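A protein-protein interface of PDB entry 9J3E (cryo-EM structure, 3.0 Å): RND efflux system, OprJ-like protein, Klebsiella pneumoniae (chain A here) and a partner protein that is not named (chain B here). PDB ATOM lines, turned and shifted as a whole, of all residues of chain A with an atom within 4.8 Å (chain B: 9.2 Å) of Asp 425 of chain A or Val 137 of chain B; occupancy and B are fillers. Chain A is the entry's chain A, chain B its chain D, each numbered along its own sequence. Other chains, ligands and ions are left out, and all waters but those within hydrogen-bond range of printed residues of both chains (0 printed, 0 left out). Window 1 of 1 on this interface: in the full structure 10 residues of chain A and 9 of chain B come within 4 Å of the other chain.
The guanidinium group of Arg 209 of chain A sits at hydrogen-bond distance from the backbone carbonyl oxygen of Ala 136 of chain B, 2.5 Å away. The side-chain hydroxyl (OH) of Tyr 419 of chain A sits at hydrogen-bond distance from the side-chain carboxylate (OD2) of Asp 135 of chain B (3.0 Å). OG of Ser 138 of chain B lies close to O of Val 423 of chain A. OD2 of Asp 425 of chain A sits close to O of Asp 135 of chain B. O of Ala 136 of chain B lies close to OD1 of Asp 425 of chain A (2.7 Å). O of Asp 135 of chain B sits close to N of Tyr 426 of chain A (3.5 Å).
Leu 131 of chain B touches Arg 209 of chain A. Val 137 of chain B touches Arg 209 of chain A. CB of Ser 138 of chain B touches C of Asp 424 of chain A, 3.8 Å away. OD1 of Asp 425 of chain A touches CA of Val 137 of chain B, at 3.3 Å. Asp 425 of chain A touches Ser 138 of chain B (N to CB, 3.7 Å).
Of the 9 printed residues of chain A, 6 touch a printed residue of chain B. Hydrophobic or aromatic side chains of chain A that line the printed part of chain B: Tyr 419 and Tyr 426. Hydrophobic or aromatic side chains of chain B that line the printed part of chain A: Leu 131 and Val 137. Among the printed residues, 11 pairs touch across the chains. Among the printed residues, no Asp or Glu carboxylate lies within 4 Å of a Lys or Arg side-chain nitrogen of the other chain.
Asp 425 of chain A touches just these residues of chain B: Asp 135, Ala 136, Val 137 and Ser 138. Val 137 of chain B touches two residues of chain A. Of the printed residues of chain B, Tyr 426 of chain A touches Asp 135. Of the printed residues of chain B, Tyr 419 of chain A touches Asp 135 (3.0 Å). Of the printed residues of chain A, Asp 135 of chain B touches Tyr 419, Asp 425 and Tyr 426. Of the printed residues of chain A, Ala 136 of chain B touches Arg 209 and Asp 425. Gln 140 of chain B touches none of the printed residues of chain A. The nearest residue of chain B that does not touch Asp 425 of chain A is Asp 141 of chain B (5.3 Å). The nearest printed residue of chain A that does not touch Ala 136 of chain B is Leu 427 of chain A (4.7 Å).
The guanidinium group of Arg 209 of chain A is in salt-bridge range of the side-chain carboxylate of Asp 425 of chain A. The backbone NH of Leu 427 of chain A sits close to the side-chain carboxylate of Asp 425 of chain A, at 3.4 Å. The backbone NH of Ala 136 of chain B lies within hydrogen-bond range of the backbone carbonyl oxygen of Leu 131 of chain B (2.8 Å). The side-chain hydroxyl of Ser 138 of chain B sits close to the backbone NH of Gln 140 of chain B. OG of Ser 138 of chain B lies within hydrogen-bond range of OD2 of Asp 141 of chain B (2.7 Å).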
ATOM      1  N   ARG A 209     -19.112  -2.959  18.585  1.00  0.00           N
ATOM      2  CA  ARG A 209     -19.955  -2.024  19.320  1.00  0.00           C
ATOM      3  C   ARG A 209     -19.160  -0.817  19.800  1.00  0.00           C
ATOM      4  O   ARG A 209     -19.622   0.324  19.702  1.00  0.00           O
ATOM      5  CB  ARG A 209     -20.610  -2.742  20.493  1.00  0.00           C
ATOM      6  CG  ARG A 209     -21.190  -1.811  21.506  1.00  0.00           C
ATOM      7  CD  ARG A 209     -21.704  -2.575  22.690  1.00  0.00           C
ATOM      8  NE  ARG A 209     -22.949  -3.252  22.367  1.00  0.00           N
ATOM      9  CZ  ARG A 209     -23.994  -3.298  23.178  1.00  0.00           C
ATOM     10  NH1 ARG A 209     -23.980  -2.697  24.355  1.00  0.00           N
ATOM     11  NH2 ARG A 209     -25.081  -3.958  22.796  1.00  0.00           N
ATOM     12  N   TYR A 419     -33.694 -14.129  22.001  1.00  0.00           N
ATOM     13  CA  TYR A 419     -32.847 -13.493  21.000  1.00  0.00           C
ATOM     14  C   TYR A 419     -33.497 -13.526  19.626  1.00  0.00           C
ATOM     15  O   TYR A 419     -33.563 -12.501  18.941  1.00  0.00           O
ATOM     16  CB  TYR A 419     -31.487 -14.182  20.964  1.00  0.00           C
ATOM     17  CG  TYR A 419     -30.719 -13.960  19.687  1.00  0.00           C
ATOM     18  CD1 TYR A 419     -30.462 -12.684  19.215  1.00  0.00           C
ATOM     19  CD2 TYR A 419     -30.273 -15.033  18.940  1.00  0.00           C
ATOM     20  CE1 TYR A 419     -29.767 -12.488  18.046  1.00  0.00           C
ATOM     21  CE2 TYR A 419     -29.581 -14.846  17.772  1.00  0.00           C
ATOM     22  CZ  TYR A 419     -29.331 -13.574  17.328  1.00  0.00           C
ATOM     23  OH  TYR A 419     -28.638 -13.391  16.159  1.00  0.00           O
ATOM     24  N   VAL A 423     -35.822  -9.629  21.470  1.00  0.00           N
ATOM     25  CA  VAL A 423     -35.869  -8.984  22.772  1.00  0.00           C
ATOM     26  C   VAL A 423     -34.488  -8.892  23.402  1.00  0.00           C
ATOM     27  O   VAL A 423     -34.093  -7.828  23.878  1.00  0.00           O
ATOM     28  CB  VAL A 423     -36.853  -9.723  23.699  1.00  0.00           C
ATOM     29  CG1 VAL A 423     -36.624  -9.315  25.133  1.00  0.00           C
ATOM     30  CG2 VAL A 423     -38.269  -9.413  23.290  1.00  0.00           C
ATOM     31  N   ASP A 424     -33.736  -9.983  23.403  1.00  0.00           N
ATOM     32  CA  ASP A 424     -32.411 -10.004  23.995  1.00  0.00           C
ATOM     33  C   ASP A 424     -31.345  -9.813  22.930  1.00  0.00           C
ATOM     34  O   ASP A 424     -31.527 -10.170  21.764  1.00  0.00           O
ATOM     35  CB  ASP A 424     -32.152 -11.312  24.743  1.00  0.00           C
ATOM     36  CG  ASP A 424     -32.812 -11.342  26.103  1.00  0.00           C
ATOM     37  OD1 ASP A 424     -33.340 -10.298  26.534  1.00  0.00           O
ATOM     38  OD2 ASP A 424     -32.801 -12.412  26.747  1.00  0.00           O
ATOM     39  N   ASP A 425     -30.225  -9.250  23.356  1.00  0.00           N
ATOM     40  CA  ASP A 425     -29.073  -9.032  22.506  1.00  0.00           C
ATOM     41  C   ASP A 425     -28.413 -10.361  22.162  1.00  0.00           C
ATOM     42  O   ASP A 425     -28.654 -11.388  22.797  1.00  0.00           O
ATOM     43  CB  ASP A 425     -28.080  -8.119  23.212  1.00  0.00           C
ATOM     44  CG  ASP A 425     -27.168  -7.405  22.258  1.00  0.00           C
ATOM     45  OD1 ASP A 425     -26.833  -6.238  22.532  1.00  0.00           O
ATOM     46  OD2 ASP A 425     -26.786  -8.011  21.238  1.00  0.00           O
ATOM     47  N   TYR A 426     -27.565 -10.338  21.134  1.00  0.00           N
ATOM     48  CA  TYR A 426     -26.741 -11.510  20.864  1.00  0.00           C
ATOM     49  C   TYR A 426     -25.749 -11.771  21.986  1.00  0.00           C
ATOM     50  O   TYR A 426     -25.338 -12.918  22.188  1.00  0.00           O
ATOM     51  CB  TYR A 426     -26.002 -11.356  19.544  1.00  0.00           C
ATOM     52  CG  TYR A 426     -25.529 -12.668  18.982  1.00  0.00           C
ATOM     53  CD1 TYR A 426     -24.213 -12.838  18.587  1.00  0.00           C
ATOM     54  CD2 TYR A 426     -26.387 -13.745  18.868  1.00  0.00           C
ATOM     55  CE1 TYR A 426     -23.768 -14.036  18.082  1.00  0.00           C
ATOM     56  CE2 TYR A 426     -25.953 -14.949  18.361  1.00  0.00           C
ATOM     57  CZ  TYR A 426     -24.642 -15.089  17.971  1.00  0.00           C
ATOM     58  OH  TYR A 426     -24.201 -16.288  17.466  1.00  0.00           O
ATOM     59  N   LEU A 427     -25.348 -10.731  22.717  1.00  0.00           N
ATOM     60  CA  LEU A 427     -24.451 -10.933  23.850  1.00  0.00           C
ATOM     61  C   LEU A 427     -25.087 -11.832  24.897  1.00  0.00           C
ATOM     62  O   LEU A 427     -24.425 -12.713  25.452  1.00  0.00           O
ATOM     63  CB  LEU A 427     -24.069  -9.593  24.476  1.00  0.00           C
ATOM     64  CG  LEU A 427     -22.899  -8.774  23.927  1.00  0.00           C
ATOM     65  CD1 LEU A 427     -21.602  -9.239  24.555  1.00  0.00           C
ATOM     66  CD2 LEU A 427     -22.815  -8.841  22.433  1.00  0.00           C
ATOM     67  N   ARG A 428     -26.371 -11.617  25.185  1.00  0.00           N
ATOM     68  CA  ARG A 428     -27.061 -12.458  26.156  1.00  0.00           C
ATOM     69  C   ARG A 428     -27.122 -13.905  25.694  1.00  0.00           C
ATOM     70  O   ARG A 428     -26.911 -14.829  26.489  1.00  0.00           O
ATOM     71  CB  ARG A 428     -28.463 -11.915  26.407  1.00  0.00           C
ATOM     72  CG  ARG A 428     -28.482 -10.572  27.102  1.00  0.00           C
ATOM     73  CD  ARG A 428     -28.221 -10.722  28.595  1.00  0.00           C
ATOM     74  NE  ARG A 428     -28.956 -11.841  29.176  1.00  0.00           N
ATOM     75  CZ  ARG A 428     -28.426 -13.019  29.479  1.00  0.00           C
ATOM     76  NH1 ARG A 428     -27.141 -13.269  29.296  1.00  0.00           N
ATOM     77  NH2 ARG A 428     -29.209 -13.973  29.978  1.00  0.00           N
ATOM     78  N   TYR A 429     -27.415 -14.126  24.415  1.00  0.00           N
ATOM     79  CA  TYR A 429     -27.459 -15.489  23.903  1.00  0.00           C
ATOM     80  C   TYR A 429     -26.093 -16.151  23.984  1.00  0.00           C
ATOM     81  O   TYR A 429     -25.980 -17.322  24.367  1.00  0.00           O
ATOM     82  CB  TYR A 429     -27.974 -15.486  22.470  1.00  0.00           C
ATOM     83  CG  TYR A 429     -27.829 -16.809  21.780  1.00  0.00           C
ATOM     84  CD1 TYR A 429     -26.773 -17.051  20.922  1.00  0.00           C
ATOM     85  CD2 TYR A 429     -28.736 -17.826  22.004  1.00  0.00           C
ATOM     86  CE1 TYR A 429     -26.635 -18.259  20.292  1.00  0.00           C
ATOM     87  CE2 TYR A 429     -28.606 -19.039  21.381  1.00  0.00           C
ATOM     88  CZ  TYR A 429     -27.556 -19.251  20.525  1.00  0.00           C
ATOM     89  OH  TYR A 429     -27.420 -20.466  19.898  1.00  0.00           O
ATOM     90  N   MET B 124     -28.045   8.423  18.192  1.00  0.00           N
ATOM     91  CA  MET B 124     -28.365   7.090  18.692  1.00  0.00           C
ATOM     92  C   MET B 124     -28.748   6.149  17.561  1.00  0.00           C
ATOM     93  O   MET B 124     -28.239   5.027  17.477  1.00  0.00           O
ATOM     94  CB  MET B 124     -29.503   7.170  19.702  1.00  0.00           C
ATOM     95  CG  MET B 124     -29.970   5.827  20.203  1.00  0.00           C
ATOM     96  SD  MET B 124     -30.215   5.786  21.977  1.00  0.00           S
ATOM     97  CE  MET B 124     -28.553   5.444  22.516  1.00  0.00           C
ATOM     98  N   VAL B 125     -29.649   6.587  16.686  1.00  0.00           N
ATOM     99  CA  VAL B 125     -30.117   5.706  15.625  1.00  0.00           C
ATOM    100  C   VAL B 125     -29.002   5.431  14.631  1.00  0.00           C
ATOM    101  O   VAL B 125     -28.867   4.311  14.128  1.00  0.00           O
ATOM    102  CB  VAL B 125     -31.361   6.300  14.944  1.00  0.00           C
ATOM    103  CG1 VAL B 125     -31.595   5.641  13.604  1.00  0.00           C
ATOM    104  CG2 VAL B 125     -32.567   6.120  15.834  1.00  0.00           C
ATOM    105  N   ARG B 127     -25.846   5.223  15.265  1.00  0.00           N
ATOM    106  CA  ARG B 127     -24.928   4.239  15.823  1.00  0.00           C
ATOM    107  C   ARG B 127     -25.568   2.863  15.906  1.00  0.00           C
ATOM    108  O   ARG B 127     -24.896   1.850  15.697  1.00  0.00           O
ATOM    109  CB  ARG B 127     -24.435   4.682  17.193  1.00  0.00           C
ATOM    110  CG  ARG B 127     -23.284   5.638  17.098  1.00  0.00           C
ATOM    111  CD  ARG B 127     -22.893   6.176  18.444  1.00  0.00           C
ATOM    112  NE  ARG B 127     -23.835   7.176  18.910  1.00  0.00           N
ATOM    113  CZ  ARG B 127     -23.499   8.212  19.660  1.00  0.00           C
ATOM    114  NH1 ARG B 127     -22.245   8.425  20.017  1.00  0.00           N
ATOM    115  NH2 ARG B 127     -24.443   9.058  20.059  1.00  0.00           N
ATOM    116  N   TYR B 128     -26.862   2.803  16.208  1.00  0.00           N
ATOM    117  CA  TYR B 128     -27.522   1.516  16.371  1.00  0.00           C
ATOM    118  C   TYR B 128     -27.791   0.820  15.048  1.00  0.00           C
ATOM    119  O   TYR B 128     -27.847  -0.413  15.013  1.00  0.00           O
ATOM    120  CB  TYR B 128     -28.838   1.699  17.121  1.00  0.00           C
ATOM    121  CG  TYR B 128     -28.692   1.631  18.616  1.00  0.00           C
ATOM    122  CD1 TYR B 128     -27.465   1.833  19.217  1.00  0.00           C
ATOM    123  CD2 TYR B 128     -29.783   1.387  19.426  1.00  0.00           C
ATOM    124  CE1 TYR B 128     -27.326   1.780  20.582  1.00  0.00           C
ATOM    125  CE2 TYR B 128     -29.654   1.332  20.792  1.00  0.00           C
ATOM    126  CZ  TYR B 128     -28.424   1.530  21.365  1.00  0.00           C
ATOM    127  OH  TYR B 128     -28.294   1.474  22.730  1.00  0.00           O
ATOM    128  N   GLU B 129     -27.952   1.575  13.966  1.00  0.00           N
ATOM    129  CA  GLU B 129     -28.340   0.978  12.691  1.00  0.00           C
ATOM    130  C   GLU B 129     -27.328  -0.031  12.167  1.00  0.00           C
ATOM    131  O   GLU B 129     -27.748  -1.124  11.752  1.00  0.00           O
ATOM    132  CB  GLU B 129     -28.608   2.096  11.682  1.00  0.00           C
ATOM    133  CG  GLU B 129     -29.385   1.673  10.463  1.00  0.00           C
ATOM    134  CD  GLU B 129     -29.386   2.747   9.402  1.00  0.00           C
ATOM    135  OE1 GLU B 129     -29.148   3.921   9.755  1.00  0.00           O
ATOM    136  OE2 GLU B 129     -29.619   2.424   8.220  1.00  0.00           O
ATOM    137  N   PRO B 130     -26.021   0.241  12.141  1.00  0.00           N
ATOM    138  CA  PRO B 130     -25.093  -0.814  11.722  1.00  0.00           C
ATOM    139  C   PRO B 130     -24.961  -1.919  12.744  1.00  0.00           C
ATOM    140  O   PRO B 130     -24.664  -3.059  12.375  1.00  0.00           O
ATOM    141  CB  PRO B 130     -23.771  -0.063  11.531  1.00  0.00           C
ATOM    142  CG  PRO B 130     -23.867   1.072  12.448  1.00  0.00           C
ATOM    143  CD  PRO B 130     -25.304   1.495  12.419  1.00  0.00           C
ATOM    144  N   LEU B 131     -25.182  -1.618  14.023  1.00  0.00           N
ATOM    145  CA  LEU B 131     -25.004  -2.633  15.050  1.00  0.00           C
ATOM    146  C   LEU B 131     -26.148  -3.631  15.063  1.00  0.00           C
ATOM    147  O   LEU B 131     -25.923  -4.824  15.286  1.00  0.00           O
ATOM    148  CB  LEU B 131     -24.864  -1.974  16.416  1.00  0.00           C
ATOM    149  CG  LEU B 131     -23.609  -1.130  16.599  1.00  0.00           C
ATOM    150  CD1 LEU B 131     -23.578  -0.537  17.986  1.00  0.00           C
ATOM    151  CD2 LEU B 131     -22.383  -1.971  16.354  1.00  0.00           C
ATOM    152  N   VAL B 132     -27.378  -3.173  14.831  1.00  0.00           N
ATOM    153  CA  VAL B 132     -28.512  -4.085  14.911  1.00  0.00           C
ATOM    154  C   VAL B 132     -28.462  -5.111  13.789  1.00  0.00           C
ATOM    155  O   VAL B 132     -28.991  -6.219  13.929  1.00  0.00           O
ATOM    156  CB  VAL B 132     -29.834  -3.299  14.906  1.00  0.00           C
ATOM    157  CG1 VAL B 132     -30.101  -2.713  13.540  1.00  0.00           C
ATOM    158  CG2 VAL B 132     -30.974  -4.190  15.335  1.00  0.00           C
ATOM    159  N   LYS B 133     -27.832  -4.772  12.663  1.00  0.00           N
ATOM    160  CA  LYS B 133     -27.738  -5.729  11.569  1.00  0.00           C
ATOM    161  C   LYS B 133     -26.857  -6.913  11.936  1.00  0.00           C
ATOM    162  O   LYS B 133     -27.128  -8.039  11.507  1.00  0.00           O
ATOM    163  CB  LYS B 133     -27.215  -5.045  10.308  1.00  0.00           C
ATOM    164  CG  LYS B 133     -28.265  -4.206   9.596  1.00  0.00           C
ATOM    165  CD  LYS B 133     -27.824  -3.778   8.202  1.00  0.00           C
ATOM    166  CE  LYS B 133     -26.330  -3.512   8.110  1.00  0.00           C
ATOM    167  NZ  LYS B 133     -25.890  -2.431   9.030  1.00  0.00           N
ATOM    168  N   ILE B 134     -25.802  -6.686  12.717  1.00  0.00           N
ATOM    169  CA  ILE B 134     -24.983  -7.770  13.237  1.00  0.00           C
ATOM    170  C   ILE B 134     -25.437  -8.201  14.624  1.00  0.00           C
ATOM    171  O   ILE B 134     -24.706  -8.910  15.318  1.00  0.00           O
ATOM    172  CB  ILE B 134     -23.496  -7.392  13.253  1.00  0.00           C
ATOM    173  CG1 ILE B 134     -23.281  -6.131  14.082  1.00  0.00           C
ATOM    174  CG2 ILE B 134     -22.998  -7.178  11.845  1.00  0.00           C
ATOM    175  CD1 ILE B 134     -21.835  -5.765  14.255  1.00  0.00           C
ATOM    176  N   ASP B 135     -26.625  -7.774  15.046  1.00  0.00           N
ATOM    177  CA  ASP B 135     -27.207  -8.163  16.327  1.00  0.00           C
ATOM    178  C   ASP B 135     -26.342  -7.734  17.503  1.00  0.00           C
ATOM    179  O   ASP B 135     -26.361  -8.364  18.559  1.00  0.00           O
ATOM    180  CB  ASP B 135     -27.464  -9.669  16.376  1.00  0.00           C
ATOM    181  CG  ASP B 135     -28.269 -10.154  15.195  1.00  0.00           C
ATOM    182  OD1 ASP B 135     -29.397  -9.660  15.003  1.00  0.00           O
ATOM    183  OD2 ASP B 135     -27.768 -11.021  14.450  1.00  0.00           O
ATOM    184  N   ALA B 136     -25.575  -6.657  17.338  1.00  0.00           N
ATOM    185  CA  ALA B 136     -24.806  -6.133  18.457  1.00  0.00           C
ATOM    186  C   ALA B 136     -25.685  -5.418  19.469  1.00  0.00           C
ATOM    187  O   ALA B 136     -25.251  -5.204  20.603  1.00  0.00           O
ATOM    188  CB  ALA B 136     -23.717  -5.188  17.959  1.00  0.00           C
ATOM    189  N   VAL B 137     -26.896  -5.025  19.078  1.00  0.00           N
ATOM    190  CA  VAL B 137     -27.886  -4.476  19.991  1.00  0.00           C
ATOM    191  C   VAL B 137     -29.202  -5.186  19.728  1.00  0.00           C
ATOM    192  O   VAL B 137     -29.489  -5.620  18.611  1.00  0.00           O
ATOM    193  CB  VAL B 137     -28.058  -2.953  19.835  1.00  0.00           C
ATOM    194  CG1 VAL B 137     -26.789  -2.238  20.237  1.00  0.00           C
ATOM    195  CG2 VAL B 137     -28.431  -2.614  18.414  1.00  0.00           C
ATOM    196  N   SER B 138     -30.005  -5.307  20.777  1.00  0.00           N
ATOM    197  CA  SER B 138     -31.256  -6.035  20.655  1.00  0.00           C
ATOM    198  C   SER B 138     -32.203  -5.305  19.716  1.00  0.00           C
ATOM    199  O   SER B 138     -32.198  -4.076  19.625  1.00  0.00           O
ATOM    200  CB  SER B 138     -31.910  -6.208  22.021  1.00  0.00           C
ATOM    201  OG  SER B 138     -32.615  -5.042  22.392  1.00  0.00           O
ATOM    202  N   GLN B 139     -33.015  -6.082  18.998  1.00  0.00           N
ATOM    203  CA  GLN B 139     -34.020  -5.488  18.127  1.00  0.00           C
ATOM    204  C   GLN B 139     -34.957  -4.587  18.916  1.00  0.00           C
ATOM    205  O   GLN B 139     -35.417  -3.561  18.402  1.00  0.00           O
ATOM    206  CB  GLN B 139     -34.810  -6.589  17.428  1.00  0.00           C
ATOM    207  CG  GLN B 139     -35.750  -6.103  16.358  1.00  0.00           C
ATOM    208  CD  GLN B 139     -35.013  -5.625  15.134  1.00  0.00           C
ATOM    209  OE1 GLN B 139     -34.007  -6.211  14.739  1.00  0.00           O
ATOM    210  NE2 GLN B 139     -35.508  -4.558  14.521  1.00  0.00           N
ATOM    211  N   GLN B 140     -35.236  -4.949  20.168  1.00  0.00           N
ATOM    212  CA  GLN B 140     -36.028  -4.088  21.037  1.00  0.00           C
ATOM    213  C   GLN B 140     -35.359  -2.741  21.236  1.00  0.00           C
ATOM    214  O   GLN B 140     -36.017  -1.697  21.175  1.00  0.00           O
ATOM    215  CB  GLN B 140     -36.239  -4.766  22.388  1.00  0.00           C
ATOM    216  CG  GLN B 140     -37.670  -5.111  22.703  1.00  0.00           C
ATOM    217  CD  GLN B 140     -38.567  -3.902  22.694  1.00  0.00           C
ATOM    218  OE1 GLN B 140     -38.113  -2.772  22.862  1.00  0.00           O
ATOM    219  NE2 GLN B 140     -39.856  -4.130  22.503  1.00  0.00           N
ATOM    220  N   ASP B 141     -34.052  -2.742  21.488  1.00  0.00           N
ATOM    221  CA  ASP B 141     -33.345  -1.488  21.703  1.00  0.00           C
ATOM    222  C   ASP B 141     -33.343  -0.641  20.445  1.00  0.00           C
ATOM    223  O   ASP B 141     -33.475   0.585  20.516  1.00  0.00           O
ATOM    224  CB  ASP B 141     -31.918  -1.758  22.169  1.00  0.00           C
ATOM    225  CG  ASP B 141     -31.865  -2.321  23.571  1.00  0.00           C
ATOM    226  OD1 ASP B 141     -32.607  -1.824  24.440  1.00  0.00           O
ATOM    227  OD2 ASP B 141     -31.078  -3.262  23.804  1.00  0.00           O
ATOM    228  N   PHE B 142     -33.189  -1.268  19.283  1.00  0.00           N
ATOM    229  CA  PHE B 142     -33.205  -0.495  18.049  1.00  0.00           C
ATOM    230  C   PHE B 142     -34.576   0.104  17.796  1.00  0.00           C
ATOM    231  O   PHE B 142     -34.686   1.248  17.347  1.00  0.00           O
ATOM    232  CB  PHE B 142     -32.789  -1.353  16.864  1.00  0.00           C
ATOM    233  CG  PHE B 142     -32.845  -0.623  15.565  1.00  0.00           C
ATOM    234  CD1 PHE B 142     -31.978   0.420  15.315  1.00  0.00           C
ATOM    235  CD2 PHE B 142     -33.775  -0.957  14.605  1.00  0.00           C
ATOM    236  CE1 PHE B 142     -32.024   1.104  14.129  1.00  0.00           C
ATOM    237  CE2 PHE B 142     -33.826  -0.274  13.414  1.00  0.00           C
ATOM    238  CZ  PHE B 142     -32.949   0.758  13.177  1.00  0.00           C
ATOM    239  N   ASP B 143     -35.638  -0.656  18.060  1.00  0.00           N
ATOM    240  CA  ASP B 143     -36.974  -0.101  17.888  1.00  0.00           C
ATOM    241  C   ASP B 143     -37.232   1.023  18.880  1.00  0.00           C
ATOM    242  O   ASP B 143     -37.890   2.010  18.543  1.00  0.00           O
ATOM    243  CB  ASP B 143     -38.024  -1.198  18.019  1.00  0.00           C
ATOM    244  CG  ASP B 143     -38.176  -2.003  16.749  1.00  0.00           C
ATOM    245  OD1 ASP B 143     -37.655  -1.561  15.707  1.00  0.00           O
ATOM    246  OD2 ASP B 143     -38.814  -3.073  16.789  1.00  0.00           O
ATOM    247  N   ASN B 144     -36.717   0.898  20.102  1.00  0.00           N
ATOM    248  CA  ASN B 144     -36.832   1.991  21.061  1.00  0.00           C
ATOM    249  C   ASN B 144     -36.090   3.226  20.575  1.00  0.00           C
ATOM    250  O   ASN B 144     -36.578   4.349  20.722  1.00  0.00           O
ATOM    251  CB  ASN B 144     -36.299   1.556  22.422  1.00  0.00           C
ATOM    252  CG  ASN B 144     -37.263   0.672  23.159  1.00  0.00           C
ATOM    253  OD1 ASN B 144     -38.447   0.628  22.841  1.00  0.00           O
ATOM    254  ND2 ASN B 144     -36.764  -0.041  24.156  1.00  0.00           N
ATOM    255  N   ALA B 145     -34.902   3.039  20.002  1.00  0.00           N
ATOM    256  CA  ALA B 145     -34.153   4.173  19.474  1.00  0.00           C
ATOM    257  C   ALA B 145     -34.893   4.828  18.319  1.00  0.00           C
ATOM    258  O   ALA B 145     -34.925   6.057  18.209  1.00  0.00           O
ATOM    259  CB  ALA B 145     -32.766   3.721  19.030  1.00  0.00           C
